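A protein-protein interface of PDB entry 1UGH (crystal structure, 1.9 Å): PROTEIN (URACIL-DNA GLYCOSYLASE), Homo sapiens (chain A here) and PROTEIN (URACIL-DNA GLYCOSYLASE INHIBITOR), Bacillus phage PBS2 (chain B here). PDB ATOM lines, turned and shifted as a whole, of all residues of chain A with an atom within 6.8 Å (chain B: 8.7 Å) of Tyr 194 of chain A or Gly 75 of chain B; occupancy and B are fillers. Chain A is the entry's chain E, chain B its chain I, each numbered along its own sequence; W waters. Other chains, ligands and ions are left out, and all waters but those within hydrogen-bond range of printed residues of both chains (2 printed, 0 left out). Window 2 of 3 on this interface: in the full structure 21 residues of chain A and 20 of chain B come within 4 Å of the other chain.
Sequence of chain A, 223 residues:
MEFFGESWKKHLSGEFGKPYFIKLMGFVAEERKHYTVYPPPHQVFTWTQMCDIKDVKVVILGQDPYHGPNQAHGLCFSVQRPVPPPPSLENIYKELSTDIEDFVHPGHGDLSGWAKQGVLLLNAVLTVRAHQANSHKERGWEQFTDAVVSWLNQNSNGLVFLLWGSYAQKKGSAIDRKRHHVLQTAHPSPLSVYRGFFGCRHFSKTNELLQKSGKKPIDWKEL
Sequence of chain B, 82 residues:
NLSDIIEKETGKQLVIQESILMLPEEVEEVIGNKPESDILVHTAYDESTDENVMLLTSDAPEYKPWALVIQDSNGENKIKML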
ATOM      1  N   ASN A  91      22.366  19.653 -10.010  1.00  0.00           N
ATOM      2  CA  ASN A  91      23.519  19.227  -9.218  1.00  0.00           C
ATOM      3  C   ASN A  91      24.017  17.859  -9.694  1.00  0.00           C
ATOM      4  O   ASN A  91      25.214  17.585  -9.672  1.00  0.00           O
ATOM      5  CB  ASN A  91      23.196  19.238  -7.727  1.00  0.00           C
ATOM      6  CG  ASN A  91      23.214  20.648  -7.137  1.00  0.00           C
ATOM      7  OD1 ASN A  91      23.525  21.620  -7.832  1.00  0.00           O
ATOM      8  ND2 ASN A  91      22.873  20.766  -5.867  1.00  0.00           N
ATOM      9  N   ALA A 186      24.830  11.462   0.175  1.00  0.00           N
ATOM     10  CA  ALA A 186      23.827  12.485   0.441  1.00  0.00           C
ATOM     11  C   ALA A 186      23.005  12.789  -0.815  1.00  0.00           C
ATOM     12  O   ALA A 186      23.449  12.529  -1.932  1.00  0.00           O
ATOM     13  CB  ALA A 186      24.510  13.745   0.946  1.00  0.00           C
ATOM     14  N   HIS A 187      21.811  13.352  -0.618  1.00  0.00           N
ATOM     15  CA  HIS A 187      20.887  13.698  -1.709  1.00  0.00           C
ATOM     16  C   HIS A 187      21.442  14.906  -2.491  1.00  0.00           C
ATOM     17  O   HIS A 187      22.031  15.809  -1.888  1.00  0.00           O
ATOM     18  CB  HIS A 187      19.509  14.039  -1.113  1.00  0.00           C
ATOM     19  CG  HIS A 187      18.409  14.175  -2.123  1.00  0.00           C
ATOM     20  ND1 HIS A 187      18.166  15.342  -2.820  1.00  0.00           N
ATOM     21  CD2 HIS A 187      17.472  13.290  -2.547  1.00  0.00           C
ATOM     22  CE1 HIS A 187      17.134  15.172  -3.629  1.00  0.00           C
ATOM     23  NE2 HIS A 187      16.692  13.935  -3.481  1.00  0.00           N
ATOM     24  N   SER A 189      20.152  17.517  -3.453  1.00  0.00           N
ATOM     25  CA  SER A 189      19.464  18.759  -3.151  1.00  0.00           C
ATOM     26  C   SER A 189      20.489  19.764  -2.634  1.00  0.00           C
ATOM     27  O   SER A 189      21.430  19.389  -1.936  1.00  0.00           O
ATOM     28  CB  SER A 189      18.412  18.515  -2.062  1.00  0.00           C
ATOM     29  OG  SER A 189      18.010  19.717  -1.422  1.00  0.00           O
ATOM     30  N   PRO A 190      20.345  21.047  -3.004  1.00  0.00           N
ATOM     31  CA  PRO A 190      21.275  22.075  -2.541  1.00  0.00           C
ATOM     32  C   PRO A 190      21.532  21.985  -1.034  1.00  0.00           C
ATOM     33  O   PRO A 190      22.642  22.224  -0.576  1.00  0.00           O
ATOM     34  CB  PRO A 190      20.545  23.360  -2.900  1.00  0.00           C
ATOM     35  CG  PRO A 190      19.934  23.006  -4.210  1.00  0.00           C
ATOM     36  CD  PRO A 190      19.377  21.620  -3.959  1.00  0.00           C
ATOM     37  N   LEU A 191      20.536  21.572  -0.261  1.00  0.00           N
ATOM     38  CA  LEU A 191      20.752  21.495   1.171  1.00  0.00           C
ATOM     39  C   LEU A 191      21.836  20.484   1.540  1.00  0.00           C
ATOM     40  O   LEU A 191      22.701  20.785   2.345  1.00  0.00           O
ATOM     41  CB  LEU A 191      19.462  21.167   1.912  1.00  0.00           C
ATOM     42  CG  LEU A 191      19.473  21.584   3.384  1.00  0.00           C
ATOM     43  CD1 LEU A 191      19.217  23.087   3.473  1.00  0.00           C
ATOM     44  CD2 LEU A 191      18.420  20.818   4.159  1.00  0.00           C
ATOM     45  N   SER A 192      21.823  19.302   0.933  1.00  0.00           N
ATOM     46  CA  SER A 192      22.813  18.272   1.261  1.00  0.00           C
ATOM     47  C   SER A 192      23.879  17.988   0.205  1.00  0.00           C
ATOM     48  O   SER A 192      24.766  17.168   0.411  1.00  0.00           O
ATOM     49  CB  SER A 192      22.082  16.974   1.608  1.00  0.00           C
ATOM     50  OG  SER A 192      20.985  16.740   0.732  1.00  0.00           O
ATOM     51  N   VAL A 193      23.839  18.721  -0.894  1.00  0.00           N
ATOM     52  CA  VAL A 193      24.771  18.497  -1.975  1.00  0.00           C
ATOM     53  C   VAL A 193      26.229  18.518  -1.571  1.00  0.00           C
ATOM     54  O   VAL A 193      27.018  17.717  -2.060  1.00  0.00           O
ATOM     55  CB  VAL A 193      24.522  19.464  -3.125  1.00  0.00           C
ATOM     56  CG1 VAL A 193      25.037  20.844  -2.795  1.00  0.00           C
ATOM     57  CG2 VAL A 193      25.109  18.907  -4.389  1.00  0.00           C
ATOM     58  N   TYR A 194      26.587  19.405  -0.653  1.00  0.00           N
ATOM     59  CA  TYR A 194      27.970  19.496  -0.207  1.00  0.00           C
ATOM     60  C   TYR A 194      28.314  18.498   0.893  1.00  0.00           C
ATOM     61  O   TYR A 194      29.468  18.380   1.298  1.00  0.00           O
ATOM     62  CB  TYR A 194      28.294  20.923   0.223  1.00  0.00           C
ATOM     63  CG  TYR A 194      28.385  21.892  -0.932  1.00  0.00           C
ATOM     64  CD1 TYR A 194      29.516  21.921  -1.758  1.00  0.00           C
ATOM     65  CD2 TYR A 194      27.356  22.787  -1.198  1.00  0.00           C
ATOM     66  CE1 TYR A 194      29.620  22.830  -2.821  1.00  0.00           C
ATOM     67  CE2 TYR A 194      27.447  23.697  -2.258  1.00  0.00           C
ATOM     68  CZ  TYR A 194      28.584  23.714  -3.059  1.00  0.00           C
ATOM     69  OH  TYR A 194      28.691  24.653  -4.060  1.00  0.00           O
ATOM     70  N   ARG A 195      27.315  17.739   1.335  1.00  0.00           N
ATOM     71  CA  ARG A 195      27.505  16.736   2.383  1.00  0.00           C
ATOM     72  C   ARG A 195      28.031  15.402   1.854  1.00  0.00           C
ATOM     73  O   ARG A 195      28.122  14.430   2.609  1.00  0.00           O
ATOM     74  CB  ARG A 195      26.195  16.481   3.135  1.00  0.00           C
ATOM     75  CG  ARG A 195      25.671  17.654   3.936  1.00  0.00           C
ATOM     76  CD  ARG A 195      26.545  17.936   5.138  1.00  0.00           C
ATOM     77  NE  ARG A 195      26.527  16.845   6.106  1.00  0.00           N
ATOM     78  CZ  ARG A 195      27.286  16.808   7.196  1.00  0.00           C
ATOM     79  NH1 ARG A 195      28.116  17.820   7.431  1.00  0.00           N
ATOM     80  NH2 ARG A 195      27.151  15.817   8.079  1.00  0.00           N
ATOM     81  N   GLY A 196      28.345  15.334   0.563  1.00  0.00           N
ATOM     82  CA  GLY A 196      28.848  14.090   0.020  1.00  0.00           C
ATOM     83  C   GLY A 196      28.539  13.796  -1.430  1.00  0.00           C
ATOM     84  O   GLY A 196      29.300  13.077  -2.074  1.00  0.00           O
ATOM     85  N   PHE A 197      27.433  14.314  -1.952  1.00  0.00           N
ATOM     86  CA  PHE A 197      27.096  14.052  -3.343  1.00  0.00           C
ATOM     87  C   PHE A 197      28.193  14.560  -4.289  1.00  0.00           C
ATOM     88  O   PHE A 197      28.721  13.787  -5.088  1.00  0.00           O
ATOM     89  CB  PHE A 197      25.749  14.657  -3.705  1.00  0.00           C
ATOM     90  CG  PHE A 197      25.296  14.315  -5.085  1.00  0.00           C
ATOM     91  CD1 PHE A 197      24.744  13.068  -5.355  1.00  0.00           C
ATOM     92  CD2 PHE A 197      25.443  15.227  -6.126  1.00  0.00           C
ATOM     93  CE1 PHE A 197      24.342  12.736  -6.653  1.00  0.00           C
ATOM     94  CE2 PHE A 197      25.046  14.904  -7.426  1.00  0.00           C
ATOM     95  CZ  PHE A 197      24.498  13.662  -7.687  1.00  0.00           C
ATOM     96  N   PHE A 198      28.541  15.846  -4.184  1.00  0.00           N
ATOM     97  CA  PHE A 198      29.604  16.437  -5.010  1.00  0.00           C
ATOM     98  C   PHE A 198      30.914  15.736  -4.688  1.00  0.00           C
ATOM     99  O   PHE A 198      31.426  15.827  -3.573  1.00  0.00           O
ATOM    100  CB  PHE A 198      29.774  17.937  -4.728  1.00  0.00           C
ATOM    101  CG  PHE A 198      28.803  18.815  -5.468  1.00  0.00           C
ATOM    102  CD1 PHE A 198      28.278  18.422  -6.694  1.00  0.00           C
ATOM    103  CD2 PHE A 198      28.430  20.047  -4.944  1.00  0.00           C
ATOM    104  CE1 PHE A 198      27.397  19.244  -7.376  1.00  0.00           C
ATOM    105  CE2 PHE A 198      27.548  20.873  -5.625  1.00  0.00           C
ATOM    106  CZ  PHE A 198      27.034  20.471  -6.841  1.00  0.00           C
ATOM    107  N   VAL B  30      23.070  19.145   8.687  1.00  0.00           N
ATOM    108  CA  VAL B  30      23.200  20.287   7.807  1.00  0.00           C
ATOM    109  C   VAL B  30      22.826  21.604   8.479  1.00  0.00           C
ATOM    110  O   VAL B  30      23.565  22.579   8.391  1.00  0.00           O
ATOM    111  CB  VAL B  30      22.345  20.103   6.562  1.00  0.00           C
ATOM    112  CG1 VAL B  30      22.594  21.242   5.597  1.00  0.00           C
ATOM    113  CG2 VAL B  30      22.647  18.759   5.919  1.00  0.00           C
ATOM    114  N   ASP B  50      20.882  34.370  -8.022  1.00  0.00           N
ATOM    115  CA  ASP B  50      21.637  33.123  -8.215  1.00  0.00           C
ATOM    116  C   ASP B  50      21.641  32.361  -6.890  1.00  0.00           C
ATOM    117  O   ASP B  50      22.638  31.742  -6.490  1.00  0.00           O
ATOM    118  CB  ASP B  50      23.067  33.415  -8.680  1.00  0.00           C
ATOM    119  CG  ASP B  50      23.696  32.241  -9.399  1.00  0.00           C
ATOM    120  OD1 ASP B  50      24.169  31.294  -8.733  1.00  0.00           O
ATOM    121  OD2 ASP B  50      23.712  32.266 -10.642  1.00  0.00           O
ATOM    122  N   ASN B  52      19.660  29.650  -4.075  1.00  0.00           N
ATOM    123  CA  ASN B  52      18.756  28.527  -3.890  1.00  0.00           C
ATOM    124  C   ASN B  52      18.027  28.866  -2.596  1.00  0.00           C
ATOM    125  O   ASN B  52      18.647  28.969  -1.527  1.00  0.00           O
ATOM    126  CB  ASN B  52      19.519  27.195  -3.739  1.00  0.00           C
ATOM    127  CG  ASN B  52      19.958  26.603  -5.074  1.00  0.00           C
ATOM    128  OD1 ASN B  52      19.166  26.470  -6.005  1.00  0.00           O
ATOM    129  ND2 ASN B  52      21.218  26.220  -5.157  1.00  0.00           N
ATOM    130  N   MET B  54      15.275  27.777   0.060  1.00  0.00           N
ATOM    131  CA  MET B  54      14.611  26.564   0.518  1.00  0.00           C
ATOM    132  C   MET B  54      13.756  26.775   1.752  1.00  0.00           C
ATOM    133  O   MET B  54      14.244  27.186   2.804  1.00  0.00           O
ATOM    134  CB  MET B  54      15.636  25.475   0.818  1.00  0.00           C
ATOM    135  CG  MET B  54      16.506  25.073  -0.347  1.00  0.00           C
ATOM    136  SD  MET B  54      18.016  24.347   0.280  1.00  0.00           S
ATOM    137  CE  MET B  54      19.205  25.597  -0.226  1.00  0.00           C
ATOM    138  N   ILE B  70      18.904  29.921   2.796  1.00  0.00           N
ATOM    139  CA  ILE B  70      19.321  30.574   1.562  1.00  0.00           C
ATOM    140  C   ILE B  70      20.768  30.195   1.263  1.00  0.00           C
ATOM    141  O   ILE B  70      21.646  30.372   2.102  1.00  0.00           O
ATOM    142  CB  ILE B  70      19.232  32.121   1.676  1.00  0.00           C
ATOM    143  CG1 ILE B  70      17.855  32.553   2.190  1.00  0.00           C
ATOM    144  CG2 ILE B  70      19.495  32.764   0.313  1.00  0.00           C
ATOM    145  CD1 ILE B  70      16.764  32.514   1.148  1.00  0.00           C
ATOM    146  N   GLN B  71      21.003  29.671   0.069  1.00  0.00           N
ATOM    147  CA  GLN B  71      22.340  29.280  -0.325  1.00  0.00           C
ATOM    148  C   GLN B  71      22.780  30.157  -1.487  1.00  0.00           C
ATOM    149  O   GLN B  71      22.033  30.337  -2.455  1.00  0.00           O
ATOM    150  CB  GLN B  71      22.355  27.813  -0.735  1.00  0.00           C
ATOM    151  CG  GLN B  71      23.738  27.225  -0.892  1.00  0.00           C
ATOM    152  CD  GLN B  71      23.688  25.786  -1.358  1.00  0.00           C
ATOM    153  OE1 GLN B  71      23.758  25.507  -2.554  1.00  0.00           O
ATOM    154  NE2 GLN B  71      23.551  24.866  -0.419  1.00  0.00           N
ATOM    155  N   ASP B  72      23.974  30.729  -1.363  1.00  0.00           N
ATOM    156  CA  ASP B  72      24.541  31.616  -2.385  1.00  0.00           C
ATOM    157  C   ASP B  72      25.505  30.863  -3.298  1.00  0.00           C
ATOM    158  O   ASP B  72      25.865  29.713  -3.008  1.00  0.00           O
ATOM    159  CB  ASP B  72      25.268  32.770  -1.707  1.00  0.00           C
ATOM    160  CG  ASP B  72      26.121  32.304  -0.554  1.00  0.00           C
ATOM    161  OD1 ASP B  72      27.012  31.457  -0.786  1.00  0.00           O
ATOM    162  OD2 ASP B  72      25.870  32.750   0.588  1.00  0.00           O
ATOM    163  N   SER B  73      25.975  31.523  -4.356  1.00  0.00           N
ATOM    164  CA  SER B  73      26.878  30.897  -5.322  1.00  0.00           C
ATOM    165  C   SER B  73      28.095  30.209  -4.717  1.00  0.00           C
ATOM    166  O   SER B  73      28.443  29.102  -5.128  1.00  0.00           O
ATOM    167  CB  SER B  73      27.325  31.896  -6.395  1.00  0.00           C
ATOM    168  OG  SER B  73      26.231  32.388  -7.151  1.00  0.00           O
ATOM    169  N   ASN B  74      28.736  30.833  -3.734  1.00  0.00           N
ATOM    170  CA  ASN B  74      29.910  30.209  -3.120  1.00  0.00           C
ATOM    171  C   ASN B  74      29.589  29.026  -2.201  1.00  0.00           C
ATOM    172  O   ASN B  74      30.456  28.554  -1.461  1.00  0.00           O
ATOM    173  CB  ASN B  74      30.801  31.243  -2.417  1.00  0.00           C
ATOM    174  CG  ASN B  74      30.033  32.122  -1.451  1.00  0.00           C
ATOM    175  OD1 ASN B  74      29.967  31.838  -0.258  1.00  0.00           O
ATOM    176  ND2 ASN B  74      29.475  33.217  -1.958  1.00  0.00           N
ATOM    177  N   GLY B  75      28.348  28.545  -2.268  1.00  0.00           N
ATOM    178  CA  GLY B  75      27.925  27.394  -1.488  1.00  0.00           C
ATOM    179  C   GLY B  75      27.705  27.593  -0.003  1.00  0.00           C
ATOM    180  O   GLY B  75      27.769  26.622   0.774  1.00  0.00           O
ATOM    181  N   GLU B  76      27.414  28.829   0.393  1.00  0.00           N
ATOM    182  CA  GLU B  76      27.184  29.156   1.796  1.00  0.00           C
ATOM    183  C   GLU B  76      25.696  29.133   2.118  1.00  0.00           C
ATOM    184  O   GLU B  76      24.875  29.720   1.403  1.00  0.00           O
ATOM    185  CB  GLU B  76      27.772  30.534   2.127  1.00  0.00           C
ATOM    186  CG  GLU B  76      28.557  30.606   3.444  1.00  0.00           C
ATOM    187  CD  GLU B  76      30.013  30.161   3.301  1.00  0.00           C
ATOM    188  OE1 GLU B  76      30.261  28.930   3.219  1.00  0.00           O
ATOM    189  OE2 GLU B  76      30.907  31.046   3.291  1.00  0.00           O
ATOM    190  N   ASN B  77      25.362  28.443   3.206  1.00  0.00           N
ATOM    191  CA  ASN B  77      23.980  28.320   3.670  1.00  0.00           C
ATOM    192  C   ASN B  77      23.657  29.388   4.713  1.00  0.00           C
ATOM    193  O   ASN B  77      24.411  29.589   5.665  1.00  0.00           O
ATOM    194  CB  ASN B  77      23.719  26.922   4.251  1.00  0.00           C
ATOM    195  CG  ASN B  77      23.311  25.906   3.188  1.00  0.00           C
ATOM    196  OD1 ASN B  77      22.709  26.261   2.173  1.00  0.00           O
ATOM    197  ND2 ASN B  77      23.615  24.634   3.429  1.00  0.00           N
ATOM    198  N   LYS B  78      22.516  30.048   4.539  1.00  0.00           N
ATOM    199  CA  LYS B  78      22.069  31.103   5.439  1.00  0.00           C
ATOM    200  C   LYS B  78      20.725  30.722   6.061  1.00  0.00           C
ATOM    201  O   LYS B  78      19.654  30.987   5.510  1.00  0.00           O
ATOM    202  CB  LYS B  78      21.994  32.424   4.678  1.00  0.00           C
ATOM    203  CG  LYS B  78      23.367  32.919   4.235  1.00  0.00           C
ATOM    204  CD  LYS B  78      23.277  34.046   3.232  1.00  0.00           C
ATOM    205  CE  LYS B  78      22.935  33.521   1.855  1.00  0.00           C
ATOM    206  NZ  LYS B  78      22.684  34.630   0.895  1.00  0.00           N
HETATM  207  O   HOH W   1      23.450  23.454  -4.743  1.00  0.00           O
HETATM  208  O   HOH W   2      28.716  26.694  -6.698  1.00  0.00           O
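Ser 189 of chain A touches none of the printed residues of chain B.
Printed residues of chain B within 4 Å of Leu 191 of chain A: Val 30 and Met 54.
No residue of chain B comes within 4 Å of Val 193 of chain A.
Tyr 194 of chain A touches just one residue of chain B: Gly 75.
Of the printed residues of chain A, Val 30 of chain B touches Leu 191 and Arg 195.
Of the printed residues of chain A, Asn 52 of chain B touches Pro 190 (3.6 Å).
Of the printed residues of chain A, Gln 71 of chain B touches Pro 190 (2.8 Å).
The nearest printed residue of chain A that does not touch Gly 75 of chain B is Pro 190 of chain A (6.9 Å).
The backbone carbonyl oxygen (O) of Pro 190 of chain A is in hydrogen-bond range of the side-chain amide nitrogen (NE2) of Gln 71 of chain B.
The backbone NH (N) of Leu 191 of chain A sits close to the side-chain sulfur (SD) of Met 54 of chain B (3.8 Å).
Asn 52 of chain B touches Pro 190 of chain A.
Met 54 of chain B touches Pro 190 of chain A.
Val 30 of chain B touches Leu 191 of chain A.
CA of Gly 75 of chain B touches CE2 of Tyr 194 of chain A (3.8 Å).
CG of Arg 195 of chain A touches CG2 of Val 30 of chain B (3.8 Å).
Water W2 bridges O of Ser 73 of chain B (2.9 Å) and OH of Tyr 194 of chain A (3.3 Å).
Water W1 lies within hydrogen-bond range of the side-chain amide nitrogen (ND2) of Asn 91 of chain A (3.0 Å) and the side-chain amide oxygen (OE1) of Gln 71 of chain B (3.0 Å).
The side-chain hydroxyl (OG) of Ser 189 of chain A sits close to the backbone NH (N) of Leu 191 of chain A (3.3 Å).
The backbone carbonyl oxygen (O) of Asn 52 of chain B is in hydrogen-bond range of the backbone NH (N) of Gln 71 of chain B (2.9 Å).
The side-chain amide oxygen of Asn 77 of chain B is in hydrogen-bond range of the side-chain amide nitrogen of Gln 71 of chain B, 3.1 Å away.
Of the 13 printed residues of chain A, 4 touch a printed residue of chain B.
Hydrophobic or aromatic side chains of chain A within 4 Å of the printed part of chain B: Pro 190, Leu 191 and Tyr 194.
Of the 13 printed residues of chain B, 5 touch a printed residue of chain A.
Along chain B the printed residues that touch a printed residue of chain A span positions 30 to 75.
Among the printed residues, no Asp or Glu carboxylate lies within 4 Å of a Lys or Arg side-chain nitrogen of the other chain.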
